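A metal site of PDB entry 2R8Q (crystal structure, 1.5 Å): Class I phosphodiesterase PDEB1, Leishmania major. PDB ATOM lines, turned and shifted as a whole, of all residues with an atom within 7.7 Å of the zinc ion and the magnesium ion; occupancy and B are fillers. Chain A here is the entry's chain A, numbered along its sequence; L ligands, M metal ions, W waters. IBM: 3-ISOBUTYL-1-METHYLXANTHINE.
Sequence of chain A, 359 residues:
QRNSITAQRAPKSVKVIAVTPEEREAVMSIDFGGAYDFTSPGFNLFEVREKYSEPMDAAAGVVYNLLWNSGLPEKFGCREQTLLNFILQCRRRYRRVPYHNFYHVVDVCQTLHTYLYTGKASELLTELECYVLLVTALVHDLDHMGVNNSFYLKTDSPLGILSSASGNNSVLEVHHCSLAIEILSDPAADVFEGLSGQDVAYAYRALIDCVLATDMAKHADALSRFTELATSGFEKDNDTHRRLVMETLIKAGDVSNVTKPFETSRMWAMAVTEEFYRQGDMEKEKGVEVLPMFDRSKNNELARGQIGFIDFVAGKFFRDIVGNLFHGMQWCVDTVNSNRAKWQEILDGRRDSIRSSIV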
ATOM      1  N   TYR A  94      20.160  30.162  20.343  1.00  0.00           N
ATOM      2  CA  TYR A  94      19.472  28.931  20.738  1.00  0.00           C
ATOM      3  C   TYR A  94      18.778  28.389  19.502  1.00  0.00           C
ATOM      4  O   TYR A  94      18.179  29.146  18.723  1.00  0.00           O
ATOM      5  CB  TYR A  94      18.466  29.175  21.871  1.00  0.00           C
ATOM      6  CG  TYR A  94      19.161  29.339  23.203  1.00  0.00           C
ATOM      7  CD1 TYR A  94      19.465  30.604  23.701  1.00  0.00           C
ATOM      8  CD2 TYR A  94      19.620  28.220  23.899  1.00  0.00           C
ATOM      9  CE1 TYR A  94      20.225  30.758  24.875  1.00  0.00           C
ATOM     10  CE2 TYR A  94      20.381  28.364  25.063  1.00  0.00           C
ATOM     11  CZ  TYR A  94      20.675  29.631  25.538  1.00  0.00           C
ATOM     12  OH  TYR A  94      21.485  29.766  26.653  1.00  0.00           O
ATOM     13  N   TYR A  99      13.738  20.756  23.593  1.00  0.00           N
ATOM     14  CA  TYR A  99      13.940  21.178  24.963  1.00  0.00           C
ATOM     15  C   TYR A  99      14.991  22.256  25.209  1.00  0.00           C
ATOM     16  O   TYR A  99      14.707  23.260  25.859  1.00  0.00           O
ATOM     17  CB  TYR A  99      14.281  19.959  25.834  1.00  0.00           C
ATOM     18  CG  TYR A  99      14.428  20.271  27.302  1.00  0.00           C
ATOM     19  CD1 TYR A  99      13.321  20.525  28.104  1.00  0.00           C
ATOM     20  CD2 TYR A  99      15.695  20.347  27.892  1.00  0.00           C
ATOM     21  CE1 TYR A  99      13.466  20.828  29.451  1.00  0.00           C
ATOM     22  CE2 TYR A  99      15.841  20.654  29.225  1.00  0.00           C
ATOM     23  CZ  TYR A  99      14.735  20.887  30.007  1.00  0.00           C
ATOM     24  OH  TYR A  99      14.886  21.178  31.337  1.00  0.00           O
ATOM     25  N   HIS A 100      16.200  22.048  24.693  1.00  0.00           N
ATOM     26  CA  HIS A 100      17.265  23.017  24.918  1.00  0.00           C
ATOM     27  C   HIS A 100      17.203  24.233  24.029  1.00  0.00           C
ATOM     28  O   HIS A 100      18.181  24.603  23.361  1.00  0.00           O
ATOM     29  CB  HIS A 100      18.629  22.342  24.820  1.00  0.00           C
ATOM     30  CG  HIS A 100      18.958  21.475  25.999  1.00  0.00           C
ATOM     31  ND1 HIS A 100      18.806  20.106  25.988  1.00  0.00           N
ATOM     32  CD2 HIS A 100      19.391  21.797  27.246  1.00  0.00           C
ATOM     33  CE1 HIS A 100      19.126  19.615  27.173  1.00  0.00           C
ATOM     34  NE2 HIS A 100      19.480  20.621  27.958  1.00  0.00           N
ATOM     35  N   HIS A 104      13.946  27.133  27.663  1.00  0.00           N
ATOM     36  CA  HIS A 104      14.579  26.441  28.786  1.00  0.00           C
ATOM     37  C   HIS A 104      15.438  27.391  29.612  1.00  0.00           C
ATOM     38  O   HIS A 104      15.393  27.342  30.845  1.00  0.00           O
ATOM     39  CB  HIS A 104      15.451  25.275  28.295  1.00  0.00           C
ATOM     40  CG  HIS A 104      16.407  24.755  29.326  1.00  0.00           C
ATOM     41  ND1 HIS A 104      15.991  24.138  30.495  1.00  0.00           N
ATOM     42  CD2 HIS A 104      17.762  24.744  29.357  1.00  0.00           C
ATOM     43  CE1 HIS A 104      17.051  23.758  31.192  1.00  0.00           C
ATOM     44  NE2 HIS A 104      18.133  24.112  30.523  1.00  0.00           N
ATOM     45  N   VAL A 105      16.214  28.247  28.954  1.00  0.00           N
ATOM     46  CA  VAL A 105      17.068  29.150  29.737  1.00  0.00           C
ATOM     47  C   VAL A 105      16.270  30.275  30.371  1.00  0.00           C
ATOM     48  O   VAL A 105      16.643  30.769  31.446  1.00  0.00           O
ATOM     49  CB  VAL A 105      18.261  29.701  28.896  1.00  0.00           C
ATOM     50  CG1 VAL A 105      19.106  28.538  28.381  1.00  0.00           C
ATOM     51  CG2 VAL A 105      17.779  30.573  27.748  1.00  0.00           C
ATOM     52  N   VAL A 108      15.086  28.598  33.446  1.00  0.00           N
ATOM     53  CA  VAL A 108      16.109  28.462  34.477  1.00  0.00           C
ATOM     54  C   VAL A 108      16.381  29.811  35.149  1.00  0.00           C
ATOM     55  O   VAL A 108      16.547  29.880  36.361  1.00  0.00           O
ATOM     56  CB  VAL A 108      17.425  27.876  33.891  1.00  0.00           C
ATOM     57  CG1 VAL A 108      18.544  27.902  34.924  1.00  0.00           C
ATOM     58  CG2 VAL A 108      17.178  26.444  33.442  1.00  0.00           C
ATOM     59  N   ALA A 137      22.326  32.115  33.772  1.00  0.00           N
ATOM     60  CA  ALA A 137      21.240  31.239  33.365  1.00  0.00           C
ATOM     61  C   ALA A 137      20.933  31.378  31.873  1.00  0.00           C
ATOM     62  O   ALA A 137      20.664  30.400  31.191  1.00  0.00           O
ATOM     63  CB  ALA A 137      19.988  31.532  34.194  1.00  0.00           C
ATOM     64  N   HIS A 140      23.879  29.618  29.739  1.00  0.00           N
ATOM     65  CA  HIS A 140      24.325  28.271  30.093  1.00  0.00           C
ATOM     66  C   HIS A 140      24.134  27.108  29.118  1.00  0.00           C
ATOM     67  O   HIS A 140      24.767  26.069  29.301  1.00  0.00           O
ATOM     68  CB  HIS A 140      23.792  27.890  31.491  1.00  0.00           C
ATOM     69  CG  HIS A 140      22.511  27.123  31.477  1.00  0.00           C
ATOM     70  ND1 HIS A 140      21.276  27.728  31.370  1.00  0.00           N
ATOM     71  CD2 HIS A 140      22.272  25.788  31.570  1.00  0.00           C
ATOM     72  CE1 HIS A 140      20.332  26.801  31.396  1.00  0.00           C
ATOM     73  NE2 HIS A 140      20.910  25.616  31.512  1.00  0.00           N
ATOM     74  N   ASP A 141      23.316  27.280  28.087  1.00  0.00           N
ATOM     75  CA  ASP A 141      23.109  26.217  27.094  1.00  0.00           C
ATOM     76  C   ASP A 141      23.241  26.732  25.650  1.00  0.00           C
ATOM     77  O   ASP A 141      22.783  26.083  24.716  1.00  0.00           O
ATOM     78  CB  ASP A 141      21.722  25.568  27.249  1.00  0.00           C
ATOM     79  CG  ASP A 141      21.734  24.414  28.225  1.00  0.00           C
ATOM     80  OD1 ASP A 141      22.738  23.670  28.235  1.00  0.00           O
ATOM     81  OD2 ASP A 141      20.738  24.237  28.950  1.00  0.00           O
ATOM     82  N   LEU A 142      23.889  27.878  25.478  1.00  0.00           N
ATOM     83  CA  LEU A 142      24.039  28.462  24.135  1.00  0.00           C
ATOM     84  C   LEU A 142      24.422  27.505  23.014  1.00  0.00           C
ATOM     85  O   LEU A 142      25.403  26.776  23.108  1.00  0.00           O
ATOM     86  CB  LEU A 142      25.053  29.614  24.177  1.00  0.00           C
ATOM     87  CG  LEU A 142      24.659  30.894  24.928  1.00  0.00           C
ATOM     88  CD1 LEU A 142      25.901  31.740  25.181  1.00  0.00           C
ATOM     89  CD2 LEU A 142      23.640  31.675  24.124  1.00  0.00           C
ATOM     90  N   HIS A 144      23.023  24.799  21.932  1.00  0.00           N
ATOM     91  CA  HIS A 144      22.846  23.370  22.189  1.00  0.00           C
ATOM     92  C   HIS A 144      22.218  22.814  20.919  1.00  0.00           C
ATOM     93  O   HIS A 144      21.337  23.455  20.318  1.00  0.00           O
ATOM     94  CB  HIS A 144      21.914  23.173  23.394  1.00  0.00           C
ATOM     95  CG  HIS A 144      21.979  21.812  24.009  1.00  0.00           C
ATOM     96  ND1 HIS A 144      21.537  20.681  23.365  1.00  0.00           N
ATOM     97  CD2 HIS A 144      22.446  21.395  25.213  1.00  0.00           C
ATOM     98  CE1 HIS A 144      21.702  19.629  24.155  1.00  0.00           C
ATOM     99  NE2 HIS A 144      22.259  20.041  25.276  1.00  0.00           N
ATOM    100  N   ASN A 149      26.527  15.206  25.604  1.00  0.00           N
ATOM    101  CA  ASN A 149      27.962  15.040  25.402  1.00  0.00           C
ATOM    102  C   ASN A 149      28.342  13.659  24.900  1.00  0.00           C
ATOM    103  O   ASN A 149      29.248  13.518  24.080  1.00  0.00           O
ATOM    104  CB  ASN A 149      28.739  15.354  26.687  1.00  0.00           C
ATOM    105  CG  ASN A 149      28.741  16.830  27.036  1.00  0.00           C
ATOM    106  OD1 ASN A 149      28.659  17.686  26.165  1.00  0.00           O
ATOM    107  ND2 ASN A 149      28.862  17.134  28.322  1.00  0.00           N
ATOM    108  N   LEU A 172      29.863  20.139  25.489  1.00  0.00           N
ATOM    109  CA  LEU A 172      28.872  21.200  25.374  1.00  0.00           C
ATOM    110  C   LEU A 172      29.123  22.406  26.277  1.00  0.00           C
ATOM    111  O   LEU A 172      29.064  23.550  25.817  1.00  0.00           O
ATOM    112  CB  LEU A 172      27.484  20.633  25.676  1.00  0.00           C
ATOM    113  CG  LEU A 172      26.828  19.803  24.579  1.00  0.00           C
ATOM    114  CD1 LEU A 172      25.753  18.924  25.180  1.00  0.00           C
ATOM    115  CD2 LEU A 172      26.247  20.730  23.532  1.00  0.00           C
ATOM    116  N   GLU A 173      29.384  22.154  27.551  1.00  0.00           N
ATOM    117  CA  GLU A 173      29.573  23.246  28.505  1.00  0.00           C
ATOM    118  C   GLU A 173      30.712  24.218  28.171  1.00  0.00           C
ATOM    119  O   GLU A 173      30.574  25.422  28.368  1.00  0.00           O
ATOM    120  CB  GLU A 173      29.719  22.680  29.918  1.00  0.00           C
ATOM    121  CG  GLU A 173      28.445  21.972  30.443  1.00  0.00           C
ATOM    122  CD  GLU A 173      28.173  20.633  29.782  1.00  0.00           C
ATOM    123  OE1 GLU A 173      29.132  20.008  29.284  1.00  0.00           O
ATOM    124  OE2 GLU A 173      27.007  20.183  29.776  1.00  0.00           O
ATOM    125  N   HIS A 176      29.387  26.372  25.437  1.00  0.00           N
ATOM    126  CA  HIS A 176      28.466  27.421  25.885  1.00  0.00           C
ATOM    127  C   HIS A 176      29.253  28.606  26.465  1.00  0.00           C
ATOM    128  O   HIS A 176      28.903  29.767  26.240  1.00  0.00           O
ATOM    129  CB  HIS A 176      27.504  26.894  26.967  1.00  0.00           C
ATOM    130  CG  HIS A 176      26.768  25.640  26.586  1.00  0.00           C
ATOM    131  ND1 HIS A 176      26.173  25.453  25.360  1.00  0.00           N
ATOM    132  CD2 HIS A 176      26.488  24.525  27.316  1.00  0.00           C
ATOM    133  CE1 HIS A 176      25.550  24.286  25.344  1.00  0.00           C
ATOM    134  NE2 HIS A 176      25.732  23.707  26.521  1.00  0.00           N
ATOM    135  N   VAL A 211      28.516  27.521  34.585  1.00  0.00           N
ATOM    136  CA  VAL A 211      28.160  26.812  33.365  1.00  0.00           C
ATOM    137  C   VAL A 211      28.819  25.421  33.359  1.00  0.00           C
ATOM    138  O   VAL A 211      28.190  24.422  33.027  1.00  0.00           O
ATOM    139  CB  VAL A 211      28.598  27.578  32.099  1.00  0.00           C
ATOM    140  CG1 VAL A 211      28.268  26.766  30.853  1.00  0.00           C
ATOM    141  CG2 VAL A 211      27.902  28.917  32.036  1.00  0.00           C
ATOM    142  N   THR A 214      27.150  22.599  35.244  1.00  0.00           N
ATOM    143  CA  THR A 214      25.910  22.002  34.765  1.00  0.00           C
ATOM    144  C   THR A 214      26.075  20.676  34.023  1.00  0.00           C
ATOM    145  O   THR A 214      25.088  20.059  33.629  1.00  0.00           O
ATOM    146  CB  THR A 214      25.105  22.962  33.868  1.00  0.00           C
ATOM    147  OG1 THR A 214      25.889  23.333  32.726  1.00  0.00           O
ATOM    148  CG2 THR A 214      24.695  24.206  34.645  1.00  0.00           C
ATOM    149  N   ASP A 215      27.316  20.243  33.810  1.00  0.00           N
ATOM    150  CA  ASP A 215      27.536  18.968  33.139  1.00  0.00           C
ATOM    151  C   ASP A 215      27.132  17.877  34.121  1.00  0.00           C
ATOM    152  O   ASP A 215      27.776  17.706  35.166  1.00  0.00           O
ATOM    153  CB  ASP A 215      29.008  18.797  32.754  1.00  0.00           C
ATOM    154  CG  ASP A 215      29.278  17.462  32.064  1.00  0.00           C
ATOM    155  OD1 ASP A 215      28.324  16.680  31.886  1.00  0.00           O
ATOM    156  OD2 ASP A 215      30.438  17.205  31.685  1.00  0.00           O
ATOM    157  N   MET A 216      26.075  17.132  33.803  1.00  0.00           N
ATOM    158  CA  MET A 216      25.583  16.089  34.695  1.00  0.00           C
ATOM    159  C   MET A 216      26.552  14.942  34.954  1.00  0.00           C
ATOM    160  O   MET A 216      26.338  14.158  35.875  1.00  0.00           O
ATOM    161  CB  MET A 216      24.245  15.554  34.180  1.00  0.00           C
ATOM    162  CG  MET A 216      23.075  16.492  34.411  1.00  0.00           C
ATOM    163  SD  MET A 216      22.805  16.917  36.164  1.00  0.00           S
ATOM    164  CE  MET A 216      21.984  15.445  36.753  1.00  0.00           C
ATOM    165  N   ILE A 250      22.542  26.782  40.276  1.00  0.00           N
ATOM    166  CA  ILE A 250      22.274  26.657  38.848  1.00  0.00           C
ATOM    167  C   ILE A 250      22.000  25.200  38.492  1.00  0.00           C
ATOM    168  O   ILE A 250      21.193  24.918  37.603  1.00  0.00           O
ATOM    169  CB  ILE A 250      23.426  27.243  37.962  1.00  0.00           C
ATOM    170  CG1 ILE A 250      22.933  27.318  36.508  1.00  0.00           C
ATOM    171  CG2 ILE A 250      24.688  26.389  38.078  1.00  0.00           C
ATOM    172  CD1 ILE A 250      23.789  28.188  35.589  1.00  0.00           C
ATOM    173  N   GLY A 253      18.379  24.693  39.409  1.00  0.00           N
ATOM    174  CA  GLY A 253      17.491  25.273  38.429  1.00  0.00           C
ATOM    175  C   GLY A 253      17.451  24.438  37.154  1.00  0.00           C
ATOM    176  O   GLY A 253      16.403  24.280  36.533  1.00  0.00           O
ATOM    177  N   ASP A 254      18.607  23.891  36.784  1.00  0.00           N
ATOM    178  CA  ASP A 254      18.714  23.087  35.582  1.00  0.00           C
ATOM    179  C   ASP A 254      17.872  21.806  35.633  1.00  0.00           C
ATOM    180  O   ASP A 254      17.335  21.373  34.603  1.00  0.00           O
ATOM    181  CB  ASP A 254      20.185  22.752  35.330  1.00  0.00           C
ATOM    182  CG  ASP A 254      20.517  22.616  33.860  1.00  0.00           C
ATOM    183  OD1 ASP A 254      19.741  23.112  33.016  1.00  0.00           O
ATOM    184  OD2 ASP A 254      21.584  22.035  33.561  1.00  0.00           O
ATOM    185  N   VAL A 255      17.728  21.208  36.810  1.00  0.00           N
ATOM    186  CA  VAL A 255      16.928  19.983  36.946  1.00  0.00           C
ATOM    187  C   VAL A 255      15.636  20.241  37.739  1.00  0.00           C
ATOM    188  O   VAL A 255      15.086  19.327  38.351  1.00  0.00           O
ATOM    189  CB  VAL A 255      17.723  18.852  37.634  1.00  0.00           C
ATOM    190  CG1 VAL A 255      18.927  18.484  36.788  1.00  0.00           C
ATOM    191  CG2 VAL A 255      18.148  19.259  39.036  1.00  0.00           C
HETATM  192  N9  IBM L   1      17.428  13.677  32.278  1.00  0.00           N
HETATM  193  C8  IBM L   1      16.812  12.454  32.218  1.00  0.00           C
HETATM  194  N7  IBM L   1      15.512  12.508  32.396  1.00  0.00           N
HETATM  195  C5  IBM L   1      15.262  13.861  32.571  1.00  0.00           C
HETATM  196  C4  IBM L   1      16.425  14.592  32.497  1.00  0.00           C
HETATM  197  N3  IBM L   1      16.566  15.927  32.631  1.00  0.00           N
HETATM  198  C2  IBM L   1      15.405  16.607  32.860  1.00  0.00           C
HETATM  199  N1  IBM L   1      14.169  15.943  32.944  1.00  0.00           N
HETATM  200  C6  IBM L   1      14.103  14.578  32.803  1.00  0.00           C
HETATM  201  O6  IBM L   1      13.029  14.002  32.875  1.00  0.00           O
HETATM  202  O2  IBM L   1      15.436  17.822  32.979  1.00  0.00           O
HETATM  203  C10 IBM L   1      12.960  16.710  33.185  1.00  0.00           C
HETATM  204  C11 IBM L   1      17.856  16.596  32.523  1.00  0.00           C
HETATM  205  C12 IBM L   1      18.387  16.434  31.095  1.00  0.00           C
HETATM  206  C13 IBM L   1      17.927  17.593  30.211  1.00  0.00           C
HETATM  207  C14 IBM L   1      19.907  16.329  31.093  1.00  0.00           C
HETATM  208 ZN    ZN M   1      20.231  23.585  30.917  1.00  0.00          ZN
HETATM  209 MG    MG M   2      23.429  22.125  29.589  1.00  0.00          MG
HETATM  210  O   HOH W   1      22.079  22.520  31.260  1.00  0.00           O
HETATM  211  O   HOH W   2      24.925  23.611  30.201  1.00  0.00           O
HETATM  212  O   HOH W   3      19.671  21.397  30.542  1.00  0.00           O
HETATM  213  O   HOH W   4      24.553  20.732  30.855  1.00  0.00           O
HETATM  214  O   HOH W   5      22.105  20.487  28.914  1.00  0.00           O
HETATM  215  O   HOH W   6      24.796  21.537  27.940  1.00  0.00           O
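The backbone carbonyl oxygen of Ala 137 is in hydrogen-bond range of a ring nitrogen (ND1) of His 140 (2.7 Å). The side-chain hydroxyl (OH) of Tyr 94 lies within hydrogen-bond range of the backbone NH (N) of Asp 141. NE2 of His 176 lies close to OD1 of Asp 141. A ring nitrogen (ND1) of His 104 is in hydrogen-bond range of the side-chain hydroxyl (OH) of Tyr 99 (3.3 Å).
Along chain A the residues within 4 Å of the zinc ion span positions 104 to 254.
Of the 23 residues printed, 1 comes within 4 Å of the magnesium ion.
The side-chain carboxylate (OD2) of Asp 141 binds the zinc ion. Water W1 binds the zinc ion, 2.2 Å away. NE2 of His 104 is bound to the zinc ion, at 2.2 Å. The side-chain carboxylate (OD1) of Asp 254 is bound to the zinc ion (2.2 Å). The zinc ion is bound by a ring nitrogen (NE2) of His 140, at 2.2 Å. Water W3 binds the zinc ion (2.3 Å). The zinc ion has six donor atoms within binding distance.
The magnesium ion is bound by OD1 of Asp 141 (2.2 Å), water W1 (2.2 Å), water W4 (2.2 Å), water W2 (2.2 Å), water W5 (2.2 Å) and water W6 (2.2 Å). The magnesium ion has six donor atoms within binding distance.
Water W6 bridges NE2 of His 176 (2.8 Å) and OE2 of Glu 173 (3.2 Å). Water W4 lies within hydrogen-bond range of OE2 of Glu 173 and O of Thr 214. Water W2 bridges O of His 140 and OG1 of Thr 214.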
